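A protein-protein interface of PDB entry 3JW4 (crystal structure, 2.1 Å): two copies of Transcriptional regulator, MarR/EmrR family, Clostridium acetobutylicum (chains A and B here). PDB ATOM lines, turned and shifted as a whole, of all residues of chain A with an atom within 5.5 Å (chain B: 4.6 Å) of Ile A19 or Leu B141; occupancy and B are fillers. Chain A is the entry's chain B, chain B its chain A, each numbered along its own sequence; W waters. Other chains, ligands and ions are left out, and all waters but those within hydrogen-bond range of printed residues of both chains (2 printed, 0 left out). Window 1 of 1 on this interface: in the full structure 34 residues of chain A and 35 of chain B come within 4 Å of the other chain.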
ATOM      1  N   PRO A  14      16.275  -0.488  -8.127  1.00  0.00           N
ATOM      2  CA  PRO A  14      16.533   0.093  -6.807  1.00  0.00           C
ATOM      3  C   PRO A  14      16.274   1.582  -6.643  1.00  0.00           C
ATOM      4  O   PRO A  14      15.605   1.939  -5.677  1.00  0.00           O
ATOM      5  CB  PRO A  14      17.995  -0.237  -6.536  1.00  0.00           C
ATOM      6  CG  PRO A  14      18.350  -1.293  -7.466  1.00  0.00           C
ATOM      7  CD  PRO A  14      17.364  -1.347  -8.587  1.00  0.00           C
ATOM      8  N   TYR A  15      16.748   2.438  -7.556  1.00  0.00           N
ATOM      9  CA  TYR A  15      16.473   3.870  -7.473  1.00  0.00           C
ATOM     10  C   TYR A  15      14.972   4.157  -7.514  1.00  0.00           C
ATOM     11  O   TYR A  15      14.464   4.943  -6.693  1.00  0.00           O
ATOM     12  CB  TYR A  15      17.085   4.662  -8.627  1.00  0.00           C
ATOM     13  CG  TYR A  15      18.581   4.844  -8.677  1.00  0.00           C
ATOM     14  CD1 TYR A  15      19.309   5.327  -7.597  1.00  0.00           C
ATOM     15  CD2 TYR A  15      19.263   4.635  -9.876  1.00  0.00           C
ATOM     16  CE1 TYR A  15      20.738   5.529  -7.703  1.00  0.00           C
ATOM     17  CE2 TYR A  15      20.640   4.814  -9.973  1.00  0.00           C
ATOM     18  CZ  TYR A  15      21.366   5.292  -8.883  1.00  0.00           C
ATOM     19  OH  TYR A  15      22.724   5.468  -9.058  1.00  0.00           O
ATOM     20  N   SER A  16      14.279   3.531  -8.474  1.00  0.00           N
ATOM     21  CA  SER A  16      12.851   3.725  -8.647  1.00  0.00           C
ATOM     22  C   SER A  16      12.080   3.290  -7.400  1.00  0.00           C
ATOM     23  O   SER A  16      11.129   3.946  -6.991  1.00  0.00           O
ATOM     24  CB  SER A  16      12.337   2.905  -9.821  1.00  0.00           C
ATOM     25  OG  SER A  16      12.895   3.356 -11.019  1.00  0.00           O
ATOM     26  N   TYR A  17      12.476   2.163  -6.826  1.00  0.00           N
ATOM     27  CA  TYR A  17      11.878   1.691  -5.577  1.00  0.00           C
ATOM     28  C   TYR A  17      11.917   2.776  -4.490  1.00  0.00           C
ATOM     29  O   TYR A  17      10.909   3.055  -3.840  1.00  0.00           O
ATOM     30  CB  TYR A  17      12.585   0.449  -5.064  1.00  0.00           C
ATOM     31  CG  TYR A  17      12.032  -0.009  -3.733  1.00  0.00           C
ATOM     32  CD1 TYR A  17      10.899  -0.828  -3.667  1.00  0.00           C
ATOM     33  CD2 TYR A  17      12.596   0.426  -2.552  1.00  0.00           C
ATOM     34  CE1 TYR A  17      10.364  -1.215  -2.439  1.00  0.00           C
ATOM     35  CE2 TYR A  17      12.095   0.028  -1.329  1.00  0.00           C
ATOM     36  CZ  TYR A  17      10.977  -0.771  -1.273  1.00  0.00           C
ATOM     37  OH  TYR A  17      10.511  -1.140  -0.041  1.00  0.00           O
ATOM     38  N   LEU A  18      13.091   3.350  -4.284  1.00  0.00           N
ATOM     39  CA  LEU A  18      13.295   4.329  -3.219  1.00  0.00           C
ATOM     40  C   LEU A  18      12.582   5.620  -3.494  1.00  0.00           C
ATOM     41  O   LEU A  18      11.974   6.194  -2.588  1.00  0.00           O
ATOM     42  CB  LEU A  18      14.791   4.611  -3.000  1.00  0.00           C
ATOM     43  CG  LEU A  18      15.504   3.377  -2.459  1.00  0.00           C
ATOM     44  CD1 LEU A  18      17.004   3.448  -2.665  1.00  0.00           C
ATOM     45  CD2 LEU A  18      15.157   3.119  -0.964  1.00  0.00           C
ATOM     46  N   ILE A  19      12.660   6.086  -4.735  1.00  0.00           N
ATOM     47  CA  ILE A  19      11.960   7.278  -5.138  1.00  0.00           C
ATOM     48  C   ILE A  19      10.443   7.125  -4.907  1.00  0.00           C
ATOM     49  O   ILE A  19       9.805   8.030  -4.345  1.00  0.00           O
ATOM     50  CB  ILE A  19      12.266   7.670  -6.606  1.00  0.00           C
ATOM     51  CG1 ILE A  19      13.705   8.175  -6.721  1.00  0.00           C
ATOM     52  CG2 ILE A  19      11.306   8.769  -7.077  1.00  0.00           C
ATOM     53  CD1 ILE A  19      14.340   8.083  -8.155  1.00  0.00           C
ATOM     54  N   ARG A  20       9.869   5.976  -5.260  1.00  0.00           N
ATOM     55  CA  ARG A  20       8.402   5.786  -5.066  1.00  0.00           C
ATOM     56  C   ARG A  20       8.035   5.595  -3.593  1.00  0.00           C
ATOM     57  O   ARG A  20       6.992   6.026  -3.153  1.00  0.00           O
ATOM     58  CB  ARG A  20       7.908   4.551  -5.816  1.00  0.00           C
ATOM     59  CG  ARG A  20       8.101   4.608  -7.308  1.00  0.00           C
ATOM     60  CD  ARG A  20       7.841   3.232  -7.925  1.00  0.00           C
ATOM     61  NE  ARG A  20       6.647   3.216  -8.771  1.00  0.00           N
ATOM     62  CZ  ARG A  20       6.635   2.884 -10.066  1.00  0.00           C
ATOM     63  NH1 ARG A  20       7.757   2.521 -10.709  1.00  0.00           N
ATOM     64  NH2 ARG A  20       5.484   2.897 -10.730  1.00  0.00           N
ATOM     65  N   SER A  21       8.880   4.880  -2.858  1.00  0.00           N
ATOM     66  CA  SER A  21       8.690   4.643  -1.430  1.00  0.00           C
ATOM     67  C   SER A  21       8.702   5.960  -0.657  1.00  0.00           C
ATOM     68  O   SER A  21       7.786   6.228   0.138  1.00  0.00           O
ATOM     69  CB  SER A  21       9.795   3.748  -0.914  1.00  0.00           C
ATOM     70  OG  SER A  21       9.645   3.472   0.436  1.00  0.00           O
ATOM     71  N   ILE A  22       9.712   6.787  -0.923  1.00  0.00           N
ATOM     72  CA  ILE A  22       9.794   8.118  -0.328  1.00  0.00           C
ATOM     73  C   ILE A  22       8.578   8.974  -0.744  1.00  0.00           C
ATOM     74  O   ILE A  22       7.858   9.540   0.119  1.00  0.00           O
ATOM     75  CB  ILE A  22      11.121   8.806  -0.681  1.00  0.00           C
ATOM     76  CG1 ILE A  22      12.305   8.119   0.015  1.00  0.00           C
ATOM     77  CG2 ILE A  22      11.125  10.240  -0.221  1.00  0.00           C
ATOM     78  CD1 ILE A  22      13.639   8.422  -0.662  1.00  0.00           C
ATOM     79  N   GLY A  23       8.301   9.036  -2.042  1.00  0.00           N
ATOM     80  CA  GLY A  23       7.073   9.699  -2.543  1.00  0.00           C
ATOM     81  C   GLY A  23       5.772   9.317  -1.864  1.00  0.00           C
ATOM     82  O   GLY A  23       4.941  10.182  -1.504  1.00  0.00           O
ATOM     83  N   MET A  24       5.558   8.005  -1.749  1.00  0.00           N
ATOM     84  CA  MET A  24       4.334   7.483  -1.166  1.00  0.00           C
ATOM     85  C   MET A  24       4.306   7.813   0.340  1.00  0.00           C
ATOM     86  O   MET A  24       3.233   8.133   0.882  1.00  0.00           O
ATOM     87  CB  MET A  24       4.164   5.967  -1.454  1.00  0.00           C
ATOM     88  CG  MET A  24       3.787   5.619  -2.938  1.00  0.00           C
ATOM     89  SD  MET A  24       3.387   3.703  -3.384  1.00  0.00           S
ATOM     90  CE  MET A  24       3.545   3.794  -5.336  1.00  0.00           C
ATOM     91  N   LEU A 137      21.981  16.037  -2.877  1.00  0.00           N
ATOM     92  CA  LEU A 137      20.673  15.511  -3.271  1.00  0.00           C
ATOM     93  C   LEU A 137      19.913  16.508  -4.151  1.00  0.00           C
ATOM     94  O   LEU A 137      19.258  16.115  -5.133  1.00  0.00           O
ATOM     95  CB  LEU A 137      19.821  15.177  -2.054  1.00  0.00           C
ATOM     96  CG  LEU A 137      18.437  14.555  -2.264  1.00  0.00           C
ATOM     97  CD1 LEU A 137      18.471  13.253  -3.083  1.00  0.00           C
ATOM     98  CD2 LEU A 137      17.724  14.324  -0.939  1.00  0.00           C
ATOM     99  N   LEU A 141      18.913  15.546  -7.939  1.00  0.00           N
ATOM    100  CA  LEU A 141      17.504  15.403  -8.274  1.00  0.00           C
ATOM    101  C   LEU A 141      17.098  16.400  -9.381  1.00  0.00           C
ATOM    102  O   LEU A 141      16.278  16.080 -10.237  1.00  0.00           O
ATOM    103  CB  LEU A 141      16.599  15.555  -7.050  1.00  0.00           C
ATOM    104  CG  LEU A 141      16.632  14.486  -5.944  1.00  0.00           C
ATOM    105  CD1 LEU A 141      15.765  14.975  -4.774  1.00  0.00           C
ATOM    106  CD2 LEU A 141      16.202  13.168  -6.430  1.00  0.00           C
ATOM    107  N   ILE B  19      10.844  14.928  -5.981  1.00  0.00           N
ATOM    108  CA  ILE B  19      10.495  13.533  -5.725  1.00  0.00           C
ATOM    109  C   ILE B  19       9.164  13.158  -6.372  1.00  0.00           C
ATOM    110  O   ILE B  19       9.085  12.136  -7.028  1.00  0.00           O
ATOM    111  CB  ILE B  19      10.540  13.243  -4.230  1.00  0.00           C
ATOM    112  CG1 ILE B  19      12.000  13.243  -3.799  1.00  0.00           C
ATOM    113  CG2 ILE B  19       9.934  11.883  -3.907  1.00  0.00           C
ATOM    114  CD1 ILE B  19      12.203  13.480  -2.376  1.00  0.00           C
ATOM    115  N   ILE B  22       9.662  13.290 -10.450  1.00  0.00           N
ATOM    116  CA  ILE B  22      10.376  12.135 -10.941  1.00  0.00           C
ATOM    117  C   ILE B  22       9.525  10.880 -10.766  1.00  0.00           C
ATOM    118  O   ILE B  22       9.415  10.068 -11.695  1.00  0.00           O
ATOM    119  CB  ILE B  22      11.755  11.940 -10.253  1.00  0.00           C
ATOM    120  CG1 ILE B  22      12.687  13.109 -10.569  1.00  0.00           C
ATOM    121  CG2 ILE B  22      12.365  10.617 -10.675  1.00  0.00           C
ATOM    122  CD1 ILE B  22      13.851  13.243  -9.572  1.00  0.00           C
ATOM    123  N   GLY B  23       8.908  10.730  -9.612  1.00  0.00           N
ATOM    124  CA  GLY B  23       8.035   9.580  -9.350  1.00  0.00           C
ATOM    125  C   GLY B  23       6.976   9.428 -10.426  1.00  0.00           C
ATOM    126  O   GLY B  23       6.746   8.312 -10.925  1.00  0.00           O
ATOM    127  N   LEU B  26       8.300   8.158 -13.757  1.00  0.00           N
ATOM    128  CA  LEU B  26       8.684   6.729 -13.807  1.00  0.00           C
ATOM    129  C   LEU B  26       7.621   5.884 -14.529  1.00  0.00           C
ATOM    130  O   LEU B  26       7.902   4.774 -14.970  1.00  0.00           O
ATOM    131  CB  LEU B  26       8.962   6.150 -12.417  1.00  0.00           C
ATOM    132  CG  LEU B  26      10.183   6.739 -11.692  1.00  0.00           C
ATOM    133  CD1 LEU B  26      10.228   6.262 -10.227  1.00  0.00           C
ATOM    134  CD2 LEU B  26      11.460   6.402 -12.390  1.00  0.00           C
ATOM    135  N   ILE B 125      17.737   6.739 -15.206  1.00  0.00           N
ATOM    136  CA  ILE B 125      17.879   7.680 -14.085  1.00  0.00           C
ATOM    137  C   ILE B 125      19.308   8.208 -13.983  1.00  0.00           C
ATOM    138  O   ILE B 125      19.511   9.339 -13.549  1.00  0.00           O
ATOM    139  CB  ILE B 125      17.473   7.026 -12.730  1.00  0.00           C
ATOM    140  CG1 ILE B 125      15.945   6.822 -12.701  1.00  0.00           C
ATOM    141  CG2 ILE B 125      17.910   7.875 -11.536  1.00  0.00           C
ATOM    142  CD1 ILE B 125      15.458   5.801 -11.676  1.00  0.00           C
ATOM    143  N   LEU B 137      23.578   9.363  -5.019  1.00  0.00           N
ATOM    144  CA  LEU B 137      22.107   9.264  -5.088  1.00  0.00           C
ATOM    145  C   LEU B 137      21.610   8.005  -4.345  1.00  0.00           C
ATOM    146  O   LEU B 137      20.640   8.038  -3.600  1.00  0.00           O
ATOM    147  CB  LEU B 137      21.607   9.186  -6.542  1.00  0.00           C
ATOM    148  CG  LEU B 137      20.069   9.161  -6.757  1.00  0.00           C
ATOM    149  CD1 LEU B 137      19.386  10.370  -6.131  1.00  0.00           C
ATOM    150  CD2 LEU B 137      19.672   9.102  -8.238  1.00  0.00           C
ATOM    151  N   MET B 138      22.257   6.883  -4.598  1.00  0.00           N
ATOM    152  CA  MET B 138      21.871   5.628  -3.962  1.00  0.00           C
ATOM    153  C   MET B 138      22.079   5.706  -2.461  1.00  0.00           C
ATOM    154  O   MET B 138      21.170   5.402  -1.705  1.00  0.00           O
ATOM    155  CB  MET B 138      22.636   4.470  -4.554  1.00  0.00           C
ATOM    156  CG  MET B 138      22.270   3.150  -3.918  1.00  0.00           C
ATOM    157  SD  MET B 138      20.372   2.788  -4.126  1.00  0.00           S
ATOM    158  CE  MET B 138      20.522   2.195  -5.827  1.00  0.00           C
ATOM    159  N   SER B 139      23.263   6.122  -2.020  1.00  0.00           N
ATOM    160  CA  SER B 139      23.481   6.297  -0.569  1.00  0.00           C
ATOM    161  C   SER B 139      22.450   7.224   0.096  1.00  0.00           C
ATOM    162  O   SER B 139      21.928   6.941   1.177  1.00  0.00           O
ATOM    163  CB  SER B 139      24.887   6.851  -0.308  1.00  0.00           C
ATOM    164  OG  SER B 139      25.857   5.906  -0.723  1.00  0.00           O
ATOM    165  N   ILE B 140      22.140   8.334  -0.564  1.00  0.00           N
ATOM    166  CA  ILE B 140      21.301   9.329   0.071  1.00  0.00           C
ATOM    167  C   ILE B 140      19.854   8.874   0.065  1.00  0.00           C
ATOM    168  O   ILE B 140      19.160   9.013   1.075  1.00  0.00           O
ATOM    169  CB  ILE B 140      21.462  10.700  -0.568  1.00  0.00           C
ATOM    170  CG1 ILE B 140      22.893  11.182  -0.351  1.00  0.00           C
ATOM    171  CG2 ILE B 140      20.428  11.696   0.026  1.00  0.00           C
ATOM    172  CD1 ILE B 140      23.286  12.370  -1.226  1.00  0.00           C
ATOM    173  N   LEU B 141      19.401   8.284  -1.032  1.00  0.00           N
ATOM    174  CA  LEU B 141      18.037   7.803  -1.061  1.00  0.00           C
ATOM    175  C   LEU B 141      17.807   6.716  -0.005  1.00  0.00           C
ATOM    176  O   LEU B 141      16.763   6.687   0.645  1.00  0.00           O
ATOM    177  CB  LEU B 141      17.634   7.276  -2.452  1.00  0.00           C
ATOM    178  CG  LEU B 141      17.449   8.316  -3.558  1.00  0.00           C
ATOM    179  CD1 LEU B 141      17.181   7.571  -4.870  1.00  0.00           C
ATOM    180  CD2 LEU B 141      16.308   9.300  -3.241  1.00  0.00           C
ATOM    181  N   ILE B 142      18.789   5.840   0.186  1.00  0.00           N
ATOM    182  CA  ILE B 142      18.687   4.817   1.210  1.00  0.00           C
ATOM    183  C   ILE B 142      18.487   5.495   2.585  1.00  0.00           C
ATOM    184  O   ILE B 142      17.593   5.112   3.352  1.00  0.00           O
ATOM    185  CB  ILE B 142      19.907   3.883   1.200  1.00  0.00           C
ATOM    186  CG1 ILE B 142      19.923   3.036  -0.076  1.00  0.00           C
ATOM    187  CG2 ILE B 142      19.945   2.978   2.471  1.00  0.00           C
ATOM    188  CD1 ILE B 142      21.179   2.174  -0.225  1.00  0.00           C
ATOM    189  N   LYS B 143      19.321   6.494   2.883  1.00  0.00           N
ATOM    190  CA  LYS B 143      19.275   7.223   4.148  1.00  0.00           C
ATOM    191  C   LYS B 143      17.921   7.953   4.320  1.00  0.00           C
ATOM    192  O   LYS B 143      17.302   7.877   5.357  1.00  0.00           O
ATOM    193  CB  LYS B 143      20.416   8.225   4.202  1.00  0.00           C
ATOM    194  CG  LYS B 143      21.409   8.089   5.325  1.00  0.00           C
ATOM    195  CD  LYS B 143      22.490   9.228   5.285  1.00  0.00           C
ATOM    196  CE  LYS B 143      22.983   9.588   6.689  1.00  0.00           C
ATOM    197  NZ  LYS B 143      23.281  11.051   6.936  1.00  0.00           N
ATOM    198  N   VAL B 144      17.466   8.656   3.290  1.00  0.00           N
ATOM    199  CA  VAL B 144      16.180   9.327   3.346  1.00  0.00           C
ATOM    200  C   VAL B 144      15.071   8.313   3.622  1.00  0.00           C
ATOM    201  O   VAL B 144      14.300   8.496   4.572  1.00  0.00           O
ATOM    202  CB  VAL B 144      15.898  10.160   2.092  1.00  0.00           C
ATOM    203  CG1 VAL B 144      14.450  10.722   2.112  1.00  0.00           C
ATOM    204  CG2 VAL B 144      16.915  11.292   1.981  1.00  0.00           C
ATOM    205  N   ASN B 145      15.032   7.226   2.857  1.00  0.00           N
ATOM    206  CA  ASN B 145      13.986   6.240   3.036  1.00  0.00           C
ATOM    207  C   ASN B 145      14.031   5.592   4.432  1.00  0.00           C
ATOM    208  O   ASN B 145      12.988   5.299   5.047  1.00  0.00           O
ATOM    209  CB  ASN B 145      14.043   5.218   1.931  1.00  0.00           C
ATOM    210  CG  ASN B 145      12.869   4.253   1.949  1.00  0.00           C
ATOM    211  OD1 ASN B 145      11.720   4.658   1.772  1.00  0.00           O
ATOM    212  ND2 ASN B 145      13.160   2.961   2.080  1.00  0.00           N
HETATM  213  O   HOH W   1       8.173   9.702  -5.846  1.00  0.00           O
HETATM  214  O   HOH W   2      11.065   0.758   1.965  1.00  0.00           O
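OG of Ser A21 lies within hydrogen-bond range of OD1 of Asn B145, at 2.7 Å.
Ile A19 touches its own counterpart, Ile B19.
Ile A19 touches Leu B141, but with the chains exchanged Leu A141 does not touch Ile B19 (4.3 Å).
Ile A22 touches Leu B141, and with the chains exchanged Leu A141 touches Ile B22.
Gly A23 touches Ile B19, but with the chains exchanged Ile A19 does not touch Gly B23 (4.003 Å).
Positions printed for both chains: 19, 22, 23, 137 and 141.
Of the 20 pairs that touch across the chains among the printed residues, 3 have their exchanged pair printed and touching as well.
Printed residues of chain B within 4 Å of Ile A19: Ile B19 and Leu B141.
Of the printed residues of chain A, Leu B141 touches Leu A18 (3.9 Å), Ile A19 (3.98 Å) and Ile A22 (3.8 Å).
Of the printed residues of chain A, Leu B26 touches Ser A16 and Arg A20.
Printed residues of chain A within 4 Å of Ile B140: Leu A137 (3.9 Å).
Of the printed residues of chain B, Ile A22 touches Leu B141 (3.8 Å), Val B144 (3.7 Å) and Asn B145 (3.9 Å).
Of the printed residues of chain B, Ser A16 touches Leu B26 and Ile B125.
Met A24 touches none of the printed residues of chain B.
Tyr A17 touches none of the printed residues of chain B.
The nearest printed residue of chain B that does not touch Ile A19 is Gly B23 (4.003 Å).
The nearest printed residue of chain B that does not touch Ser A16 is Leu B141 (6.1 Å).
Tyr A15 touches Met B138 (CE1 to N, 3.7 Å).
Leu B26 touches Ser A16 (CD2 to OG, 3.6 Å).
CD1 of Leu A18 touches SD of Met B138, at 3.7 Å.
Ile B142 touches Leu A18.
CD2 of Leu A18 touches ND2 of Asn B145 (3.6 Å).
O of Ile A19 touches CG2 of Ile B19, 3.9 Å away.
CD1 of Leu B141 touches CG1 of Ile A19, 3.98 Å away.
Val B144 touches Ile A22 (CG1 to CD1, 3.7 Å).
CG2 of Ile B140 touches CD2 of Leu A137 (3.9 Å).
Ile B22 touches Leu A141 (CD1 to O, 3.8 Å).
Water W1 lies within hydrogen-bond range of the backbone carbonyl oxygen of Ile A19 and the backbone carbonyl oxygen of Ile B19.
Water W2 lies within hydrogen-bond range of OH of Tyr A17 (2.8 Å), ND2 of Asn B145 (3.0 Å) and OG of Ser A21 (3.4 Å).
Of the 13 printed residues of chain A, 11 touch a printed residue of chain B.
Printed residues of chain A that touch a printed residue of chain B: Pro A14, Tyr A15, Ser A16, Leu A18, Ile A19, Arg A20, Ser A21, Ile A22, Gly A23, Leu A137 and Leu A141.
Hydrophobic or aromatic side chains of chain A within 4 Å of the printed part of chain B: Pro A14, Tyr A15, Leu A18, Ile A19, Ile A22, Leu A137 and Leu A141.
Of the 14 printed residues of chain B, 11 touch a printed residue of chain A.
Printed residues of chain B that touch a printed residue of chain A: Ile B19, Ile B22, Leu B26, Ile B125, Leu B137, Met B138, Ile B140, Leu B141, Ile B142, Val B144 and Asn B145.
Along chain B the printed residues that touch a printed residue of chain A span positions 19 to 145.
Among the printed residues, 20 pairs touch across the chains.
Among the printed residues, no Asp or Glu carboxylate lies within 4 Å of a Lys or Arg side-chain nitrogen of the other chain.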
